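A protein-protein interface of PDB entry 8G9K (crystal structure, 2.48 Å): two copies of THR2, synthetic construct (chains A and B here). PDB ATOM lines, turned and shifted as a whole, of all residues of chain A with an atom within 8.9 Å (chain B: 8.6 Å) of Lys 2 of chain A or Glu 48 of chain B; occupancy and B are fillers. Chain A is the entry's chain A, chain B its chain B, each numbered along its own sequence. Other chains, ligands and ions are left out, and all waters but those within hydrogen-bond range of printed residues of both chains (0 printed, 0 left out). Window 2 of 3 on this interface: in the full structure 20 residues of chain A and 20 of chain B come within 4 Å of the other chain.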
ATOM      1  N   PRO A   1      17.214  -7.429  22.622  1.00  0.00           N
ATOM      2  CA  PRO A   1      17.435  -6.245  21.786  1.00  0.00           C
ATOM      3  C   PRO A   1      16.439  -5.132  22.091  1.00  0.00           C
ATOM      4  O   PRO A   1      16.842  -4.054  22.528  1.00  0.00           O
ATOM      5  CB  PRO A   1      17.239  -6.778  20.363  1.00  0.00           C
ATOM      6  CG  PRO A   1      17.537  -8.233  20.465  1.00  0.00           C
ATOM      7  CD  PRO A   1      17.036  -8.647  21.814  1.00  0.00           C
ATOM      8  N   LYS A   2      15.149  -5.396  21.859  1.00  0.00           N
ATOM      9  CA  LYS A   2      14.130  -4.404  22.184  1.00  0.00           C
ATOM     10  C   LYS A   2      14.068  -4.142  23.682  1.00  0.00           C
ATOM     11  O   LYS A   2      13.722  -3.032  24.105  1.00  0.00           O
ATOM     12  CB  LYS A   2      12.763  -4.855  21.670  1.00  0.00           C
ATOM     13  CG  LYS A   2      12.693  -5.053  20.166  1.00  0.00           C
ATOM     14  CD  LYS A   2      11.252  -5.076  19.675  1.00  0.00           C
ATOM     15  CE  LYS A   2      10.421  -6.102  20.427  1.00  0.00           C
ATOM     16  NZ  LYS A   2       9.031  -6.185  19.897  1.00  0.00           N
ATOM     17  N   LYS A   3      14.396  -5.146  24.497  1.00  0.00           N
ATOM     18  CA  LYS A   3      14.405  -4.949  25.943  1.00  0.00           C
ATOM     19  C   LYS A   3      15.548  -4.034  26.367  1.00  0.00           C
ATOM     20  O   LYS A   3      15.408  -3.258  27.319  1.00  0.00           O
ATOM     21  CB  LYS A   3      14.505  -6.298  26.654  1.00  0.00           C
ATOM     22  N   ILE A   4      16.682  -4.107  25.668  1.00  0.00           N
ATOM     23  CA  ILE A   4      17.837  -3.293  26.036  1.00  0.00           C
ATOM     24  C   ILE A   4      17.582  -1.823  25.723  1.00  0.00           C
ATOM     25  O   ILE A   4      17.973  -0.934  26.489  1.00  0.00           O
ATOM     26  CB  ILE A   4      19.099  -3.812  25.323  1.00  0.00           C
ATOM     27  CG1 ILE A   4      19.312  -5.296  25.622  1.00  0.00           C
ATOM     28  CG2 ILE A   4      20.320  -3.001  25.734  1.00  0.00           C
ATOM     29  CD1 ILE A   4      20.455  -5.914  24.847  1.00  0.00           C
ATOM     30  N   VAL A   5      16.918  -1.545  24.598  1.00  0.00           N
ATOM     31  CA  VAL A   5      16.716  -0.163  24.171  1.00  0.00           C
ATOM     32  C   VAL A   5      15.790   0.572  25.133  1.00  0.00           C
ATOM     33  O   VAL A   5      16.019   1.743  25.461  1.00  0.00           O
ATOM     34  CB  VAL A   5      16.178  -0.127  22.729  1.00  0.00           C
ATOM     35  CG1 VAL A   5      15.935   1.308  22.284  1.00  0.00           C
ATOM     36  CG2 VAL A   5      17.146  -0.824  21.787  1.00  0.00           C
ATOM     37  N   LYS A   6      14.734  -0.097  25.603  1.00  0.00           N
ATOM     38  CA  LYS A   6      13.785   0.553  26.501  1.00  0.00           C
ATOM     39  C   LYS A   6      14.437   0.922  27.829  1.00  0.00           C
ATOM     40  O   LYS A   6      14.210   2.018  28.354  1.00  0.00           O
ATOM     41  CB  LYS A   6      12.575  -0.351  26.729  1.00  0.00           C
ATOM     42  N   ASP A   7      15.249   0.020  28.386  1.00  0.00           N
ATOM     43  CA  ASP A   7      15.937   0.321  29.638  1.00  0.00           C
ATOM     44  C   ASP A   7      16.953   1.441  29.456  1.00  0.00           C
ATOM     45  O   ASP A   7      17.143   2.266  30.357  1.00  0.00           O
ATOM     46  CB  ASP A   7      16.620  -0.936  30.177  1.00  0.00           C
ATOM     47  CG  ASP A   7      15.637  -2.040  30.505  1.00  0.00           C
ATOM     48  OD1 ASP A   7      14.458  -1.729  30.775  1.00  0.00           O
ATOM     49  OD2 ASP A   7      16.044  -3.221  30.498  1.00  0.00           O
ATOM     50  N   ALA A   8      17.614   1.485  28.298  1.00  0.00           N
ATOM     51  CA  ALA A   8      18.621   2.512  28.057  1.00  0.00           C
ATOM     52  C   ALA A   8      17.982   3.889  27.924  1.00  0.00           C
ATOM     53  O   ALA A   8      18.439   4.858  28.540  1.00  0.00           O
ATOM     54  CB  ALA A   8      19.431   2.166  26.808  1.00  0.00           C
ATOM     55  N   LYS A   9      16.913   3.992  27.126  1.00  0.00           N
ATOM     56  CA  LYS A   9      16.260   5.281  26.918  1.00  0.00           C
ATOM     57  C   LYS A   9      15.694   5.839  28.217  1.00  0.00           C
ATOM     58  O   LYS A   9      15.745   7.051  28.455  1.00  0.00           O
ATOM     59  CB  LYS A   9      15.151   5.148  25.874  1.00  0.00           C
ATOM     60  CG  LYS A   9      15.643   4.938  24.455  1.00  0.00           C
ATOM     61  CD  LYS A   9      14.478   4.949  23.483  1.00  0.00           C
ATOM     62  CE  LYS A   9      14.956   4.945  22.045  1.00  0.00           C
ATOM     63  NZ  LYS A   9      13.816   5.034  21.092  1.00  0.00           N
ATOM     64  N   LEU A  45      23.751  -4.078  22.858  1.00  0.00           N
ATOM     65  CA  LEU A  45      22.936  -4.435  21.701  1.00  0.00           C
ATOM     66  C   LEU A  45      23.731  -5.269  20.705  1.00  0.00           C
ATOM     67  O   LEU A  45      23.194  -6.201  20.094  1.00  0.00           O
ATOM     68  CB  LEU A  45      22.395  -3.171  21.032  1.00  0.00           C
ATOM     69  CG  LEU A  45      21.294  -2.407  21.767  1.00  0.00           C
ATOM     70  CD1 LEU A  45      21.026  -1.074  21.089  1.00  0.00           C
ATOM     71  CD2 LEU A  45      20.022  -3.236  21.830  1.00  0.00           C
ATOM     72  N   GLU A  48      24.060  -8.993  22.043  1.00  0.00           N
ATOM     73  CA  GLU A  48      22.827  -9.766  22.062  1.00  0.00           C
ATOM     74  C   GLU A  48      22.168  -9.869  20.691  1.00  0.00           C
ATOM     75  O   GLU A  48      21.026 -10.327  20.599  1.00  0.00           O
ATOM     76  CB  GLU A  48      21.845  -9.163  23.071  1.00  0.00           C
ATOM     77  CG  GLU A  48      22.424  -8.980  24.469  1.00  0.00           C
ATOM     78  CD  GLU A  48      22.764 -10.294  25.151  1.00  0.00           C
ATOM     79  OE1 GLU A  48      22.242 -11.347  24.730  1.00  0.00           O
ATOM     80  OE2 GLU A  48      23.558 -10.272  26.116  1.00  0.00           O
ATOM     81  N   GLY A  49      22.860  -9.459  19.630  1.00  0.00           N
ATOM     82  CA  GLY A  49      22.334  -9.584  18.285  1.00  0.00           C
ATOM     83  C   GLY A  49      21.131  -8.706  18.008  1.00  0.00           C
ATOM     84  O   GLY A  49      20.037  -9.207  17.735  1.00  0.00           O
ATOM     85  N   ALA A  50      21.325  -7.394  18.067  1.00  0.00           N
ATOM     86  CA  ALA A  50      20.266  -6.429  17.816  1.00  0.00           C
ATOM     87  C   ALA A  50      20.298  -5.956  16.367  1.00  0.00           C
ATOM     88  O   ALA A  50      21.324  -6.024  15.686  1.00  0.00           O
ATOM     89  CB  ALA A  50      20.393  -5.230  18.760  1.00  0.00           C
ATOM     90  N   SER A  51      19.150  -5.470  15.902  1.00  0.00           N
ATOM     91  CA  SER A  51      19.057  -4.957  14.547  1.00  0.00           C
ATOM     92  C   SER A  51      19.779  -3.614  14.438  1.00  0.00           C
ATOM     93  O   SER A  51      19.867  -2.866  15.415  1.00  0.00           O
ATOM     94  CB  SER A  51      17.597  -4.794  14.131  1.00  0.00           C
ATOM     95  OG  SER A  51      16.955  -3.793  14.899  1.00  0.00           O
ATOM     96  N   LEU A  54      17.684  -0.568  15.613  1.00  0.00           N
ATOM     97  CA  LEU A  54      17.625  -0.331  17.053  1.00  0.00           C
ATOM     98  C   LEU A  54      18.887   0.364  17.551  1.00  0.00           C
ATOM     99  O   LEU A  54      18.826   1.186  18.472  1.00  0.00           O
ATOM    100  CB  LEU A  54      17.410  -1.649  17.798  1.00  0.00           C
ATOM    101  CG  LEU A  54      16.035  -2.305  17.654  1.00  0.00           C
ATOM    102  CD1 LEU A  54      15.990  -3.627  18.405  1.00  0.00           C
ATOM    103  CD2 LEU A  54      14.943  -1.370  18.148  1.00  0.00           C
ATOM    104  N   ILE A  55      20.038   0.046  16.955  1.00  0.00           N
ATOM    105  CA  ILE A  55      21.280   0.708  17.339  1.00  0.00           C
ATOM    106  C   ILE A  55      21.254   2.173  16.919  1.00  0.00           C
ATOM    107  O   ILE A  55      21.697   3.056  17.665  1.00  0.00           O
ATOM    108  CB  ILE A  55      22.488  -0.036  16.741  1.00  0.00           C
ATOM    109  CG1 ILE A  55      22.540  -1.473  17.266  1.00  0.00           C
ATOM    110  CG2 ILE A  55      23.784   0.696  17.059  1.00  0.00           C
ATOM    111  CD1 ILE A  55      23.651  -2.304  16.663  1.00  0.00           C
ATOM    112  N   ASP A  57      18.552   4.026  16.534  1.00  0.00           N
ATOM    113  CA  ASP A  57      17.572   4.723  17.362  1.00  0.00           C
ATOM    114  C   ASP A  57      18.167   5.114  18.709  1.00  0.00           C
ATOM    115  O   ASP A  57      18.028   6.259  19.153  1.00  0.00           O
ATOM    116  CB  ASP A  57      16.338   3.842  17.555  1.00  0.00           C
ATOM    117  CG  ASP A  57      15.286   4.497  18.426  1.00  0.00           C
ATOM    118  OD1 ASP A  57      15.241   5.744  18.485  1.00  0.00           O
ATOM    119  OD2 ASP A  57      14.507   3.758  19.066  1.00  0.00           O
ATOM    120  N   PRO B   1      14.791 -12.985  19.631  1.00  0.00           N
ATOM    121  CA  PRO B   1      16.161 -12.794  19.143  1.00  0.00           C
ATOM    122  C   PRO B   1      16.943 -14.102  19.095  1.00  0.00           C
ATOM    123  O   PRO B   1      16.693 -14.938  18.226  1.00  0.00           O
ATOM    124  CB  PRO B   1      16.764 -11.832  20.167  1.00  0.00           C
ATOM    125  CG  PRO B   1      16.007 -12.111  21.427  1.00  0.00           C
ATOM    126  CD  PRO B   1      14.612 -12.479  21.005  1.00  0.00           C
ATOM    127  N   LYS B   2      17.889 -14.266  20.023  1.00  0.00           N
ATOM    128  CA  LYS B   2      18.590 -15.539  20.147  1.00  0.00           C
ATOM    129  C   LYS B   2      17.633 -16.658  20.530  1.00  0.00           C
ATOM    130  O   LYS B   2      17.851 -17.819  20.162  1.00  0.00           O
ATOM    131  CB  LYS B   2      19.710 -15.421  21.181  1.00  0.00           C
ATOM    132  CG  LYS B   2      20.686 -14.281  20.920  1.00  0.00           C
ATOM    133  CD  LYS B   2      20.904 -13.435  22.168  1.00  0.00           C
ATOM    134  CE  LYS B   2      21.594 -14.224  23.271  1.00  0.00           C
ATOM    135  NZ  LYS B   2      23.011 -14.534  22.932  1.00  0.00           N
ATOM    136  N   ILE B   4      14.541 -16.922  19.477  1.00  0.00           N
ATOM    137  CA  ILE B   4      13.742 -17.293  18.313  1.00  0.00           C
ATOM    138  C   ILE B   4      14.507 -18.268  17.425  1.00  0.00           C
ATOM    139  O   ILE B   4      13.925 -19.202  16.860  1.00  0.00           O
ATOM    140  CB  ILE B   4      13.319 -16.031  17.536  1.00  0.00           C
ATOM    141  CG1 ILE B   4      12.490 -15.108  18.429  1.00  0.00           C
ATOM    142  CG2 ILE B   4      12.538 -16.408  16.287  1.00  0.00           C
ATOM    143  CD1 ILE B   4      12.074 -13.823  17.752  1.00  0.00           C
ATOM    144  N   LYS B  40       8.190 -17.907   8.759  1.00  0.00           N
ATOM    145  CA  LYS B  40       7.587 -17.259   9.919  1.00  0.00           C
ATOM    146  C   LYS B  40       8.648 -16.853  10.934  1.00  0.00           C
ATOM    147  O   LYS B  40       8.561 -15.776  11.534  1.00  0.00           O
ATOM    148  CB  LYS B  40       6.556 -18.181  10.568  1.00  0.00           C
ATOM    149  CG  LYS B  40       5.705 -17.487  11.620  1.00  0.00           C
ATOM    150  CD  LYS B  40       5.232 -18.452  12.697  1.00  0.00           C
ATOM    151  CE  LYS B  40       4.379 -19.567  12.120  1.00  0.00           C
ATOM    152  NZ  LYS B  40       3.867 -20.470  13.187  1.00  0.00           N
ATOM    153  N   ALA B  41       9.656 -17.704  11.139  1.00  0.00           N
ATOM    154  CA  ALA B  41      10.720 -17.376  12.081  1.00  0.00           C
ATOM    155  C   ALA B  41      11.579 -16.221  11.580  1.00  0.00           C
ATOM    156  O   ALA B  41      12.057 -15.413  12.385  1.00  0.00           O
ATOM    157  CB  ALA B  41      11.584 -18.607  12.346  1.00  0.00           C
ATOM    158  N   LEU B  42      11.790 -16.129  10.265  1.00  0.00           N
ATOM    159  CA  LEU B  42      12.514 -14.991   9.707  1.00  0.00           C
ATOM    160  C   LEU B  42      11.736 -13.699   9.916  1.00  0.00           C
ATOM    161  O   LEU B  42      12.293 -12.688  10.361  1.00  0.00           O
ATOM    162  CB  LEU B  42      12.789 -15.222   8.220  1.00  0.00           C
ATOM    163  CG  LEU B  42      13.788 -16.322   7.854  1.00  0.00           C
ATOM    164  CD1 LEU B  42      13.813 -16.543   6.349  1.00  0.00           C
ATOM    165  CD2 LEU B  42      15.175 -15.982   8.373  1.00  0.00           C
ATOM    166  N   LYS B  43      10.439 -13.713   9.595  1.00  0.00           N
ATOM    167  CA  LYS B  43       9.599 -12.548   9.848  1.00  0.00           C
ATOM    168  C   LYS B  43       9.512 -12.237  11.335  1.00  0.00           C
ATOM    169  O   LYS B  43       9.352 -11.073  11.719  1.00  0.00           O
ATOM    170  CB  LYS B  43       8.199 -12.772   9.274  1.00  0.00           C
ATOM    171  CG  LYS B  43       8.135 -12.779   7.756  1.00  0.00           C
ATOM    172  CD  LYS B  43       6.718 -13.055   7.275  1.00  0.00           C
ATOM    173  CE  LYS B  43       5.726 -12.064   7.865  1.00  0.00           C
ATOM    174  NZ  LYS B  43       4.330 -12.341   7.426  1.00  0.00           N
ATOM    175  N   GLU B  44       9.614 -13.261  12.185  1.00  0.00           N
ATOM    176  CA  GLU B  44       9.606 -13.025  13.623  1.00  0.00           C
ATOM    177  C   GLU B  44      10.889 -12.339  14.071  1.00  0.00           C
ATOM    178  O   GLU B  44      10.855 -11.424  14.903  1.00  0.00           O
ATOM    179  CB  GLU B  44       9.410 -14.343  14.371  1.00  0.00           C
ATOM    180  CG  GLU B  44       8.903 -14.176  15.794  1.00  0.00           C
ATOM    181  CD  GLU B  44       7.490 -13.621  15.844  1.00  0.00           C
ATOM    182  OE1 GLU B  44       6.747 -13.788  14.853  1.00  0.00           O
ATOM    183  OE2 GLU B  44       7.124 -13.016  16.873  1.00  0.00           O
ATOM    184  N   LEU B  45      12.032 -12.767  13.528  1.00  0.00           N
ATOM    185  CA  LEU B  45      13.295 -12.111  13.847  1.00  0.00           C
ATOM    186  C   LEU B  45      13.291 -10.652  13.412  1.00  0.00           C
ATOM    187  O   LEU B  45      13.886  -9.802  14.085  1.00  0.00           O
ATOM    188  CB  LEU B  45      14.457 -12.858  13.190  1.00  0.00           C
ATOM    189  CG  LEU B  45      14.842 -14.219  13.775  1.00  0.00           C
ATOM    190  CD1 LEU B  45      15.901 -14.892  12.915  1.00  0.00           C
ATOM    191  CD2 LEU B  45      15.334 -14.066  15.204  1.00  0.00           C
ATOM    192  N   LEU B  46      12.624 -10.342  12.299  1.00  0.00           N
ATOM    193  CA  LEU B  46      12.546  -8.960  11.842  1.00  0.00           C
ATOM    194  C   LEU B  46      11.696  -8.111  12.779  1.00  0.00           C
ATOM    195  O   LEU B  46      12.029  -6.952  13.050  1.00  0.00           O
ATOM    196  CB  LEU B  46      11.987  -8.910  10.419  1.00  0.00           C
ATOM    197  CG  LEU B  46      11.780  -7.515   9.828  1.00  0.00           C
ATOM    198  CD1 LEU B  46      13.107  -6.789   9.692  1.00  0.00           C
ATOM    199  CD2 LEU B  46      11.067  -7.596   8.487  1.00  0.00           C
ATOM    200  N   ARG B  47      10.595  -8.673  13.286  1.00  0.00           N
ATOM    201  CA  ARG B  47       9.712  -7.911  14.165  1.00  0.00           C
ATOM    202  C   ARG B  47      10.386  -7.590  15.492  1.00  0.00           C
ATOM    203  O   ARG B  47      10.253  -6.474  16.009  1.00  0.00           O
ATOM    204  CB  ARG B  47       8.413  -8.681  14.404  1.00  0.00           C
ATOM    205  CG  ARG B  47       7.435  -8.652  13.241  1.00  0.00           C
ATOM    206  CD  ARG B  47       6.119  -9.330  13.607  1.00  0.00           C
ATOM    207  NE  ARG B  47       5.438  -8.667  14.718  1.00  0.00           N
ATOM    208  CZ  ARG B  47       5.463  -9.093  15.977  1.00  0.00           C
ATOM    209  NH1 ARG B  47       6.136 -10.189  16.299  1.00  0.00           N
ATOM    210  NH2 ARG B  47       4.815  -8.420  16.918  1.00  0.00           N
ATOM    211  N   GLU B  48      11.111  -8.550  16.060  1.00  0.00           N
ATOM    212  CA  GLU B  48      11.719  -8.395  17.373  1.00  0.00           C
ATOM    213  C   GLU B  48      13.097  -7.745  17.319  1.00  0.00           C
ATOM    214  O   GLU B  48      13.802  -7.734  18.333  1.00  0.00           O
ATOM    215  CB  GLU B  48      11.811  -9.756  18.071  1.00  0.00           C
ATOM    216  CG  GLU B  48      10.525 -10.571  18.018  1.00  0.00           C
ATOM    217  CD  GLU B  48       9.380  -9.930  18.779  1.00  0.00           C
ATOM    218  OE1 GLU B  48       9.645  -9.139  19.709  1.00  0.00           O
ATOM    219  OE2 GLU B  48       8.211 -10.219  18.447  1.00  0.00           O
ATOM    220  N   GLY B  49      13.495  -7.210  16.168  1.00  0.00           N
ATOM    221  CA  GLY B  49      14.761  -6.512  16.047  1.00  0.00           C
ATOM    222  C   GLY B  49      15.978  -7.397  16.214  1.00  0.00           C
ATOM    223  O   GLY B  49      16.789  -7.183  17.120  1.00  0.00           O
ATOM    224  N   ALA B  50      16.122  -8.391  15.345  1.00  0.00           N
ATOM    225  CA  ALA B  50      17.268  -9.285  15.386  1.00  0.00           C
ATOM    226  C   ALA B  50      18.375  -8.776  14.467  1.00  0.00           C
ATOM    227  O   ALA B  50      18.140  -8.004  13.535  1.00  0.00           O
ATOM    228  CB  ALA B  50      16.864 -10.704  14.985  1.00  0.00           C
ATOM    229  N   SER B  51      19.596  -9.223  14.748  1.00  0.00           N
ATOM    230  CA  SER B  51      20.733  -8.834  13.933  1.00  0.00           C
ATOM    231  C   SER B  51      20.663  -9.519  12.569  1.00  0.00           C
ATOM    232  O   SER B  51      20.098 -10.609  12.442  1.00  0.00           O
ATOM    233  CB  SER B  51      22.043  -9.200  14.626  1.00  0.00           C
ATOM    234  OG  SER B  51      22.218 -10.605  14.675  1.00  0.00           O
ATOM    235  N   LEU B  54      22.048 -13.187  12.600  1.00  0.00           N
ATOM    236  CA  LEU B  54      21.118 -14.235  13.012  1.00  0.00           C
ATOM    237  C   LEU B  54      20.183 -14.617  11.871  1.00  0.00           C
ATOM    238  O   LEU B  54      19.886 -15.801  11.670  1.00  0.00           O
ATOM    239  CB  LEU B  54      20.308 -13.778  14.225  1.00  0.00           C
ATOM    240  CG  LEU B  54      21.067 -13.570  15.534  1.00  0.00           C
ATOM    241  CD1 LEU B  54      20.133 -13.016  16.598  1.00  0.00           C
ATOM    242  CD2 LEU B  54      21.696 -14.874  15.996  1.00  0.00           C
ATOM    243  N   ASP B  99      15.661  -5.433   7.420  1.00  0.00           N
ATOM    244  CA  ASP B  99      16.374  -5.376   8.690  1.00  0.00           C
ATOM    245  C   ASP B  99      17.557  -4.419   8.649  1.00  0.00           C
ATOM    246  O   ASP B  99      18.101  -4.085   9.709  1.00  0.00           O
ATOM    247  CB  ASP B  99      16.842  -6.780   9.083  1.00  0.00           C
ATOM    248  CG  ASP B  99      17.405  -6.838  10.490  1.00  0.00           C
ATOM    249  OD1 ASP B  99      16.693  -6.438  11.435  1.00  0.00           O
ATOM    250  OD2 ASP B  99      18.556  -7.295  10.654  1.00  0.00           O
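The backbone carbonyl oxygen of Gly 49 of chain A is in hydrogen-bond range of the backbone NH of Ser 51 of chain B (3.0 Å). The backbone NH (N) of Ser 51 of chain A is in hydrogen-bond range of the backbone carbonyl oxygen (O) of Gly 49 of chain B, 3.2 Å away. The side-chain carboxylate of Glu 48 of chain B lies within salt-bridge range of the side-chain amino group of Lys 2 of chain A (3.0 Å). The side-chain amino group of Lys 2 of chain B lies within salt-bridge range of the side-chain carboxylate of Glu 48 of chain A.
Among the printed residues, merely in contact across the chains: Ser 51 of chain A with Asp 99 of chain B (3.3 Å), Pro 1 of chain A with Gly 49 of chain B (3.3 Å), Ser 51 of chain A with Ala 50 of chain B (3.3 Å), Ala 50 of chain A with Ser 51 of chain B (3.4 Å), Pro 1 of chain A with Pro 1 of chain B (3.6 Å), Ala 50 of chain A with Gly 49 of chain B (3.6 Å), Gly 49 of chain A with Ala 50 of chain B (3.6 Å), Leu 54 of chain A with Gly 49 of chain B (3.9 Å), Gly 49 of chain A with Gly 49 of chain B (3.9 Å), Ala 50 of chain A with Ala 50 of chain B (3.9 Å), Ser 51 of chain A with Ser 51 of chain B (3.95 Å) and Gly 49 of chain A with Leu 54 of chain B (3.98 Å).
Pro 1 of chain B touches its own counterpart, Pro 1 of chain A. Gly 49 of chain A touches its own counterpart, Gly 49 of chain B. Gly 49 of chain A touches Ala 50 of chain B, and with the chains exchanged Ala 50 of chain A touches Gly 49 of chain B. Ala 50 of chain B touches its own counterpart, Ala 50 of chain A. Positions printed for both chains: 1, 2, 4, 45, 48, 49, 50, 51 and 54. Of the 16 pairs that touch across the chains among the printed residues, 14 have their exchanged pair printed and touching as well.
Hydrophobic or aromatic side chains of chain B within 4 Å of the printed part of chain A: Pro 1 and Leu 54. Hydrophobic or aromatic side chains of chain A that line the printed part of chain B: Pro 1 and Leu 54. Among the printed residues, 16 pairs touch across the chains. Among the printed residues, Asp or Glu carboxylates within 4 Å of a Lys or Arg side-chain nitrogen of the other chain: Lys 2 of chain A with Glu 48 of chain B and Glu 48 of chain A with Lys 2 of chain B.
The backbone NH (N) of Ala 50 of chain A is in hydrogen-bond range of the backbone carbonyl oxygen (O) of Leu 45 of chain A. OG of Ser 51 of chain B lies close to N of Leu 54 of chain B, at 3.3 Å. The guanidinium group (NH1) of Arg 47 of chain B lies within salt-bridge range of the side-chain carboxylate (OE2) of Glu 48 of chain B (3.0 Å). N of Ala 50 of chain B is in hydrogen-bond range of O of Leu 45 of chain B (2.9 Å). The side-chain hydroxyl (OG) of Ser 51 of chain A sits close to the backbone NH (N) of Leu 54 of chain A (3.4 Å).
Of the printed residues of chain B, Lys 2 of chain A touches Glu 48. Of the printed residues of chain B, Leu 54 of chain A touches Gly 49. Glu 48 of chain B touches just one residue of chain A: Lys 2 (3.0 Å). Of the printed residues of chain A, Ser 51 of chain B touches Gly 49, Ala 50 and Ser 51. Of the printed residues of chain A, Asp 99 of chain B touches Ser 51 (3.3 Å). The nearest residue of chain A that does not touch Glu 48 of chain B is Pro 1 of chain A (4.1 Å).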
